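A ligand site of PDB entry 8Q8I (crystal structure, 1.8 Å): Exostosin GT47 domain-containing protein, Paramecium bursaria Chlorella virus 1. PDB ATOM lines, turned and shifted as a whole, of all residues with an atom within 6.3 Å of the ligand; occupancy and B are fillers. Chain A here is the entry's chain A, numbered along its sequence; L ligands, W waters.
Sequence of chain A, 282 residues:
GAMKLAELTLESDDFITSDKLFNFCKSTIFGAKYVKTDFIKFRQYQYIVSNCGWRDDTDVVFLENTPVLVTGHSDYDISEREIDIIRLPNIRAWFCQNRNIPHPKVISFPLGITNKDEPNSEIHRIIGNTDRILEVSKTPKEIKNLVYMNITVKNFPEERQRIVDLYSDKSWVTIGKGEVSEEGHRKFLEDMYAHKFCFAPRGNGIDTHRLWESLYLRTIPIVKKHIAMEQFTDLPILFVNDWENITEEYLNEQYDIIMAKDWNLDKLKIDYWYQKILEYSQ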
ATOM      1  N   LYS A  36      17.700  -5.792  19.662  1.00  0.00           N
ATOM      2  CA  LYS A  36      17.511  -7.193  20.026  1.00  0.00           C
ATOM      3  C   LYS A  36      16.690  -7.897  18.952  1.00  0.00           C
ATOM      4  O   LYS A  36      15.604  -7.442  18.587  1.00  0.00           O
ATOM      5  CB  LYS A  36      16.811  -7.279  21.372  1.00  0.00           C
ATOM      6  CG  LYS A  36      17.025  -8.566  22.144  1.00  0.00           C
ATOM      7  CD  LYS A  36      16.045  -8.649  23.303  1.00  0.00           C
ATOM      8  CE  LYS A  36      16.265  -9.880  24.170  1.00  0.00           C
ATOM      9  NZ  LYS A  36      16.612 -11.088  23.385  1.00  0.00           N
ATOM     10  N   ASP A  38      14.704 -10.100  18.810  1.00  0.00           N
ATOM     11  CA  ASP A  38      13.302 -10.386  19.116  1.00  0.00           C
ATOM     12  C   ASP A  38      12.393  -9.267  18.622  1.00  0.00           C
ATOM     13  O   ASP A  38      11.296  -9.538  18.107  1.00  0.00           O
ATOM     14  CB  ASP A  38      13.133 -10.588  20.620  1.00  0.00           C
ATOM     15  CG  ASP A  38      14.128 -11.583  21.197  1.00  0.00           C
ATOM     16  OD1 ASP A  38      15.334 -11.429  20.943  1.00  0.00           O
ATOM     17  OD2 ASP A  38      13.693 -12.521  21.894  1.00  0.00           O
ATOM     18  N   HIS A  73      21.707 -10.755  21.007  1.00  0.00           N
ATOM     19  CA  HIS A  73      21.126 -11.048  22.325  1.00  0.00           C
ATOM     20  C   HIS A  73      19.973 -12.033  22.210  1.00  0.00           C
ATOM     21  O   HIS A  73      18.984 -11.954  22.950  1.00  0.00           O
ATOM     22  CB  HIS A  73      20.649  -9.771  23.016  1.00  0.00           C
ATOM     23  CG  HIS A  73      21.746  -8.933  23.586  1.00  0.00           C
ATOM     24  ND1 HIS A  73      22.319  -7.891  22.880  1.00  0.00           N
ATOM     25  CD2 HIS A  73      22.358  -8.954  24.790  1.00  0.00           C
ATOM     26  CE1 HIS A  73      23.253  -7.326  23.626  1.00  0.00           C
ATOM     27  NE2 HIS A  73      23.288  -7.950  24.786  1.00  0.00           N
ATOM     28  N   SER A  74      20.074 -12.981  21.281  1.00  0.00           N
ATOM     29  CA  SER A  74      18.955 -13.886  21.064  1.00  0.00           C
ATOM     30  C   SER A  74      19.412 -15.061  20.201  1.00  0.00           C
ATOM     31  O   SER A  74      20.369 -14.960  19.445  1.00  0.00           O
ATOM     32  CB  SER A  74      17.789 -13.168  20.390  1.00  0.00           C
ATOM     33  OG  SER A  74      16.785 -14.087  20.005  1.00  0.00           O
ATOM     34  N   ASP A  75      18.696 -16.178  20.357  1.00  0.00           N
ATOM     35  CA  ASP A  75      18.871 -17.342  19.501  1.00  0.00           C
ATOM     36  C   ASP A  75      18.044 -17.266  18.226  1.00  0.00           C
ATOM     37  O   ASP A  75      18.224 -18.106  17.343  1.00  0.00           O
ATOM     38  CB  ASP A  75      18.486 -18.619  20.267  1.00  0.00           C
ATOM     39  CG  ASP A  75      19.544 -19.039  21.262  1.00  0.00           C
ATOM     40  OD1 ASP A  75      20.703 -18.573  21.134  1.00  0.00           O
ATOM     41  OD2 ASP A  75      19.225 -19.830  22.171  1.00  0.00           O
ATOM     42  N   TYR A  76      17.143 -16.295  18.116  1.00  0.00           N
ATOM     43  CA  TYR A  76      16.419 -16.084  16.876  1.00  0.00           C
ATOM     44  C   TYR A  76      17.407 -15.803  15.744  1.00  0.00           C
ATOM     45  O   TYR A  76      18.479 -15.226  15.948  1.00  0.00           O
ATOM     46  CB  TYR A  76      15.438 -14.921  17.010  1.00  0.00           C
ATOM     47  CG  TYR A  76      14.197 -15.258  17.820  1.00  0.00           C
ATOM     48  CD1 TYR A  76      13.424 -16.365  17.526  1.00  0.00           C
ATOM     49  CD2 TYR A  76      13.805 -14.443  18.878  1.00  0.00           C
ATOM     50  CE1 TYR A  76      12.293 -16.668  18.256  1.00  0.00           C
ATOM     51  CE2 TYR A  76      12.676 -14.741  19.617  1.00  0.00           C
ATOM     52  CZ  TYR A  76      11.930 -15.849  19.307  1.00  0.00           C
ATOM     53  OH  TYR A  76      10.798 -16.139  20.040  1.00  0.00           O
ATOM     54  N   LEU A 111      28.711 -14.933  18.382  1.00  0.00           N
ATOM     55  CA  LEU A 111      27.940 -14.898  19.610  1.00  0.00           C
ATOM     56  C   LEU A 111      28.826 -14.502  20.791  1.00  0.00           C
ATOM     57  O   LEU A 111      28.408 -13.720  21.651  1.00  0.00           O
ATOM     58  CB  LEU A 111      27.286 -16.256  19.861  1.00  0.00           C
ATOM     59  CG  LEU A 111      26.125 -16.328  20.851  1.00  0.00           C
ATOM     60  CD1 LEU A 111      24.928 -15.548  20.336  1.00  0.00           C
ATOM     61  CD2 LEU A 111      25.762 -17.775  21.124  1.00  0.00           C
ATOM     62  N   ILE A 113      30.748 -14.409  24.223  1.00  0.00           N
ATOM     63  CA  ILE A 113      30.605 -14.867  25.600  1.00  0.00           C
ATOM     64  C   ILE A 113      29.337 -14.257  26.187  1.00  0.00           C
ATOM     65  O   ILE A 113      28.908 -13.176  25.787  1.00  0.00           O
ATOM     66  CB  ILE A 113      31.836 -14.478  26.458  1.00  0.00           C
ATOM     67  CG1 ILE A 113      33.130 -14.998  25.825  1.00  0.00           C
ATOM     68  CG2 ILE A 113      31.697 -15.017  27.880  1.00  0.00           C
ATOM     69  CD1 ILE A 113      33.198 -16.502  25.714  1.00  0.00           C
ATOM     70  N   THR A 114      28.746 -14.969  27.140  1.00  0.00           N
ATOM     71  CA  THR A 114      27.534 -14.493  27.781  1.00  0.00           C
ATOM     72  C   THR A 114      27.745 -13.122  28.401  1.00  0.00           C
ATOM     73  O   THR A 114      28.867 -12.754  28.789  1.00  0.00           O
ATOM     74  CB  THR A 114      27.072 -15.495  28.855  1.00  0.00           C
ATOM     75  OG1 THR A 114      26.896 -16.786  28.259  1.00  0.00           O
ATOM     76  CG2 THR A 114      25.767 -15.061  29.478  1.00  0.00           C
ATOM     77  N   ASN A 115      26.669 -12.359  28.495  1.00  0.00           N
ATOM     78  CA  ASN A 115      26.716 -11.012  29.070  1.00  0.00           C
ATOM     79  C   ASN A 115      26.596 -11.117  30.582  1.00  0.00           C
ATOM     80  O   ASN A 115      25.518 -11.410  31.121  1.00  0.00           O
ATOM     81  CB  ASN A 115      25.599 -10.150  28.470  1.00  0.00           C
ATOM     82  CG  ASN A 115      25.610 -10.144  26.960  1.00  0.00           C
ATOM     83  OD1 ASN A 115      26.551  -9.655  26.333  1.00  0.00           O
ATOM     84  ND2 ASN A 115      24.568 -10.705  26.364  1.00  0.00           N
ATOM     85  N   GLU A 118      23.744  -9.103  32.656  1.00  0.00           N
ATOM     86  CA  GLU A 118      22.320  -9.312  32.444  1.00  0.00           C
ATOM     87  C   GLU A 118      21.576  -9.074  33.770  1.00  0.00           C
ATOM     88  O   GLU A 118      21.964  -9.650  34.791  1.00  0.00           O
ATOM     89  CB  GLU A 118      22.061 -10.722  31.936  1.00  0.00           C
ATOM     90  CG  GLU A 118      20.607 -10.994  31.575  1.00  0.00           C
ATOM     91  CD  GLU A 118      20.128 -10.188  30.384  1.00  0.00           C
ATOM     92  OE1 GLU A 118      18.963  -9.743  30.389  1.00  0.00           O
ATOM     93  OE2 GLU A 118      20.916  -9.997  29.437  1.00  0.00           O
ATOM     94  N   ILE A 123      23.281 -17.104  36.524  1.00  0.00           N
ATOM     95  CA  ILE A 123      23.901 -17.902  35.470  1.00  0.00           C
ATOM     96  C   ILE A 123      24.673 -17.018  34.513  1.00  0.00           C
ATOM     97  O   ILE A 123      25.786 -17.370  34.083  1.00  0.00           O
ATOM     98  CB  ILE A 123      22.825 -18.746  34.737  1.00  0.00           C
ATOM     99  CG1 ILE A 123      23.490 -19.632  33.679  1.00  0.00           C
ATOM    100  CG2 ILE A 123      21.787 -17.846  34.099  1.00  0.00           C
ATOM    101  CD1 ILE A 123      22.534 -20.624  33.039  1.00  0.00           C
ATOM    102  N   HIS A 124      24.118 -15.864  34.153  1.00  0.00           N
ATOM    103  CA  HIS A 124      24.853 -14.908  33.336  1.00  0.00           C
ATOM    104  C   HIS A 124      26.064 -14.377  34.080  1.00  0.00           C
ATOM    105  O   HIS A 124      27.165 -14.286  33.511  1.00  0.00           O
ATOM    106  CB  HIS A 124      23.936 -13.759  32.908  1.00  0.00           C
ATOM    107  CG  HIS A 124      22.898 -14.159  31.903  1.00  0.00           C
ATOM    108  ND1 HIS A 124      21.820 -14.955  32.226  1.00  0.00           N
ATOM    109  CD2 HIS A 124      22.768 -13.864  30.588  1.00  0.00           C
ATOM    110  CE1 HIS A 124      21.073 -15.130  31.150  1.00  0.00           C
ATOM    111  NE2 HIS A 124      21.628 -14.477  30.145  1.00  0.00           N
ATOM    112  N   ILE A 127      28.655 -17.754  33.956  1.00  0.00           N
ATOM    113  CA  ILE A 127      29.248 -18.133  32.683  1.00  0.00           C
ATOM    114  C   ILE A 127      29.588 -16.942  31.813  1.00  0.00           C
ATOM    115  O   ILE A 127      30.275 -17.103  30.790  1.00  0.00           O
ATOM    116  CB  ILE A 127      28.321 -19.107  31.925  1.00  0.00           C
ATOM    117  CG1 ILE A 127      27.138 -18.380  31.272  1.00  0.00           C
ATOM    118  CG2 ILE A 127      27.805 -20.198  32.860  1.00  0.00           C
ATOM    119  CD1 ILE A 127      26.346 -19.268  30.318  1.00  0.00           C
ATOM    120  N   ASN A 155      18.930 -28.574  24.172  1.00  0.00           N
ATOM    121  CA  ASN A 155      18.988 -27.320  23.421  1.00  0.00           C
ATOM    122  C   ASN A 155      18.851 -27.556  21.924  1.00  0.00           C
ATOM    123  O   ASN A 155      18.359 -26.664  21.210  1.00  0.00           O
ATOM    124  CB  ASN A 155      20.292 -26.584  23.724  1.00  0.00           C
ATOM    125  CG  ASN A 155      20.360 -26.090  25.153  1.00  0.00           C
ATOM    126  OD1 ASN A 155      19.394 -26.194  25.911  1.00  0.00           O
ATOM    127  ND2 ASN A 155      21.508 -25.546  25.545  1.00  0.00           N
ATOM    128  N   GLY A 203      22.716 -25.223  19.223  1.00  0.00           N
ATOM    129  CA  GLY A 203      21.749 -25.418  20.287  1.00  0.00           C
ATOM    130  C   GLY A 203      20.388 -24.863  19.927  1.00  0.00           C
ATOM    131  O   GLY A 203      19.921 -25.043  18.800  1.00  0.00           O
ATOM    132  N   ASN A 204      19.737 -24.187  20.875  1.00  0.00           N
ATOM    133  CA  ASN A 204      18.479 -23.517  20.577  1.00  0.00           C
ATOM    134  C   ASN A 204      18.641 -22.572  19.402  1.00  0.00           C
ATOM    135  O   ASN A 204      17.790 -22.503  18.511  1.00  0.00           O
ATOM    136  CB  ASN A 204      17.979 -22.776  21.819  1.00  0.00           C
ATOM    137  CG  ASN A 204      16.638 -22.115  21.602  1.00  0.00           C
ATOM    138  OD1 ASN A 204      15.642 -22.771  21.283  1.00  0.00           O
ATOM    139  ND2 ASN A 204      16.589 -20.803  21.790  1.00  0.00           N
ATOM    140  N   GLY A 205      19.741 -21.814  19.379  1.00  0.00           N
ATOM    141  CA  GLY A 205      20.135 -21.057  18.221  1.00  0.00           C
ATOM    142  C   GLY A 205      21.288 -21.738  17.515  1.00  0.00           C
ATOM    143  O   GLY A 205      21.947 -22.620  18.071  1.00  0.00           O
ATOM    144  N   HIS A 209      27.622 -20.412  22.554  1.00  0.00           N
ATOM    145  CA  HIS A 209      28.726 -19.845  23.311  1.00  0.00           C
ATOM    146  C   HIS A 209      29.889 -20.810  23.429  1.00  0.00           C
ATOM    147  O   HIS A 209      31.045 -20.382  23.505  1.00  0.00           O
ATOM    148  CB  HIS A 209      28.244 -19.433  24.707  1.00  0.00           C
ATOM    149  CG  HIS A 209      27.496 -18.144  24.727  1.00  0.00           C
ATOM    150  ND1 HIS A 209      26.132 -18.071  24.912  1.00  0.00           N
ATOM    151  CD2 HIS A 209      27.920 -16.860  24.590  1.00  0.00           C
ATOM    152  CE1 HIS A 209      25.750 -16.812  24.875  1.00  0.00           C
ATOM    153  NE2 HIS A 209      26.816 -16.056  24.683  1.00  0.00           N
HETATM  154  C1  LIG L   1      21.765 -18.004  28.227  1.00  0.00           C
HETATM  155  O1  LIG L   1      20.492 -17.333  28.193  1.00  0.00           O
HETATM  156  C2  LIG L   1      20.133 -16.831  26.922  1.00  0.00           C
HETATM  157  C3  LIG L   1      18.964 -18.729  25.969  1.00  0.00           C
HETATM  158  C4  LIG L   1      19.441 -20.142  25.718  1.00  0.00           C
HETATM  159  C5  LIG L   1      18.650 -22.480  25.148  1.00  0.00           C
HETATM  160  C6  LIG L   1      16.906 -19.283  24.691  1.00  0.00           C
HETATM  161  C7  LIG L   1      17.836 -15.995  24.159  1.00  0.00           C
HETATM  162  C8  LIG L   1      17.380 -14.645  24.692  1.00  0.00           C
HETATM  163  C9  LIG L   1      15.863 -14.569  24.772  1.00  0.00           C
HETATM  164  C10 LIG L   1      15.248 -14.958  23.434  1.00  0.00           C
HETATM  165  C11 LIG L   1      15.760 -16.331  23.022  1.00  0.00           C
HETATM  166  C12 LIG L   1      15.246 -16.780  21.676  1.00  0.00           C
HETATM  167  C13 LIG L   1      18.046 -18.292  24.840  1.00  0.00           C
HETATM  168  C14 LIG L   1      18.251 -21.075  25.532  1.00  0.00           C
HETATM  169  C15 LIG L   1      21.932 -18.554  29.613  1.00  0.00           C
HETATM  170  C16 LIG L   1      22.868 -17.026  27.828  1.00  0.00           C
HETATM  171  C17 LIG L   1      22.554 -16.418  26.471  1.00  0.00           C
HETATM  172  C18 LIG L   1      21.162 -15.801  26.470  1.00  0.00           C
HETATM  173  C19 LIG L   1      14.780 -19.480  25.714  1.00  0.00           C
HETATM  174  C20 LIG L   1      14.301 -20.525  26.698  1.00  0.00           C
HETATM  175  C21 LIG L   1      14.336 -20.053  28.147  1.00  0.00           C
HETATM  176  C22 LIG L   1      14.753 -21.133  29.137  1.00  0.00           C
HETATM  177  C23 LIG L   1      16.263 -21.322  29.242  1.00  0.00           C
HETATM  178  C24 LIG L   1      16.699 -22.537  30.028  1.00  0.00           C
HETATM  179  C25 LIG L   1      16.450 -22.443  31.525  1.00  0.00           C
HETATM  180  C26 LIG L   1      16.777 -23.718  32.259  1.00  0.00           C
HETATM  181  O2  LIG L   1      17.938 -14.429  25.991  1.00  0.00           O
HETATM  182  O3  LIG L   1      15.461 -13.260  25.127  1.00  0.00           O
HETATM  183  O4  LIG L   1      15.592 -14.004  22.438  1.00  0.00           O
HETATM  184  O5  LIG L   1      17.194 -16.291  22.931  1.00  0.00           O
HETATM  185  O6  LIG L   1      15.378 -18.193  21.501  1.00  0.00           O
HETATM  186  O7  LIG L   1      17.530 -16.988  25.116  1.00  0.00           O
HETATM  187  O8  LIG L   1      16.184 -19.280  25.885  1.00  0.00           O
HETATM  188  O9  LIG L   1      17.413 -20.582  24.463  1.00  0.00           O
HETATM  189  O10 LIG L   1      20.274 -20.178  24.568  1.00  0.00           O
HETATM  190  O11 LIG L   1      20.109 -17.870  25.978  1.00  0.00           O
HETATM  191  O12 LIG L   1      24.118 -17.705  27.770  1.00  0.00           O
HETATM  192  O13 LIG L   1      23.519 -15.412  26.160  1.00  0.00           O
HETATM  193  O14 LIG L   1      21.117 -14.667  27.328  1.00  0.00           O
HETATM  194  O   HOH W   1      24.354 -12.987  27.109  1.00  0.00           O
HETATM  195  O   HOH W   2      20.043 -12.673  26.084  1.00  0.00           O
HETATM  196  O   HOH W   3      17.479 -14.269  28.598  1.00  0.00           O
HETATM  197  O   HOH W   4      21.907 -11.572  27.224  1.00  0.00           O
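NZ of Lys 36 is in hydrogen-bond range of O3 of the ligand, at 3.0 Å.
An oxygen (O4) of the ligand is in hydrogen-bond range of the side-chain carboxylate (OD2) of Asp 38 (2.5 Å).
An oxygen (O9) of the ligand lies within hydrogen-bond range of the side-chain amide nitrogen (ND2) of Asn 204, 2.8 Å away.
A ring nitrogen (NE2) of His 124 sits at hydrogen-bond distance from an oxygen (O14) of the ligand, 2.9 Å away.
An oxygen (O4) of the ligand lies within hydrogen-bond range of the side-chain hydroxyl (OG) of Ser 74, at 2.7 Å.
The side-chain hydroxyl (OG1) of Thr 114 is in hydrogen-bond range of an oxygen (O12) of the ligand, 3.0 Å away.
The side-chain carboxylate (OD2) of Asp 75 lies within hydrogen-bond range of an oxygen (O10) of the ligand, at 2.6 Å.
An oxygen (O5) of the ligand is in hydrogen-bond range of the backbone NH of Asp 75, at 3.0 Å.
His 73 touches the ligand.
Tyr 76 touches the ligand.
CD1 of Ile 127 touches O12 of the ligand (3.7 Å).
Asn 155 touches the ligand (OD1 to C5, 3.9 Å).
His 209 touches the ligand.
Hydrophobic or aromatic side chains that line the ligand: Tyr 76, His 124, Ile 127 and His 209.
Of the 19 residues printed, 12 come within 4 Å of the ligand.
Along chain A the residues within 4 Å of the ligand span positions 36 to 209.
The backbone NH of Gly 205 sits close to the side-chain carboxylate of Asp 75.
ND2 of Asn 115 lies close to NE2 of His 73 (3.4 Å).
The backbone carbonyl oxygen (O) of His 73 is in hydrogen-bond range of the side-chain amino group (NZ) of Lys 36, at 2.6 Å.
OD2 of Asp 75 lies within hydrogen-bond range of ND2 of Asn 204 (2.8 Å).
O of Asn 155 sits at hydrogen-bond distance from N of Asn 204 (2.9 Å).
The side-chain hydroxyl (OG) of Ser 74 sits at hydrogen-bond distance from the backbone NH (N) of Tyr 76 (2.9 Å).
The side-chain amino group of Lys 36 lies within salt-bridge range of the side-chain carboxylate of Asp 38, 2.8 Å away.
NE2 of His 209 sits close to N of Thr 114.
Water W2 bridges O14 of the ligand (2.6 Å) and O of His 73 (3.4 Å).
Water W1 bridges ND2 of Asn 115 (2.4 Å) and O13 of the ligand (2.7 Å).
Water W4 lies within hydrogen-bond range of the side-chain carboxylate (OE2) of Glu 118 (2.9 Å), the side-chain amide nitrogen (ND2) of Asn 115 (2.9 Å) and an oxygen (O14) of the ligand (3.2 Å).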
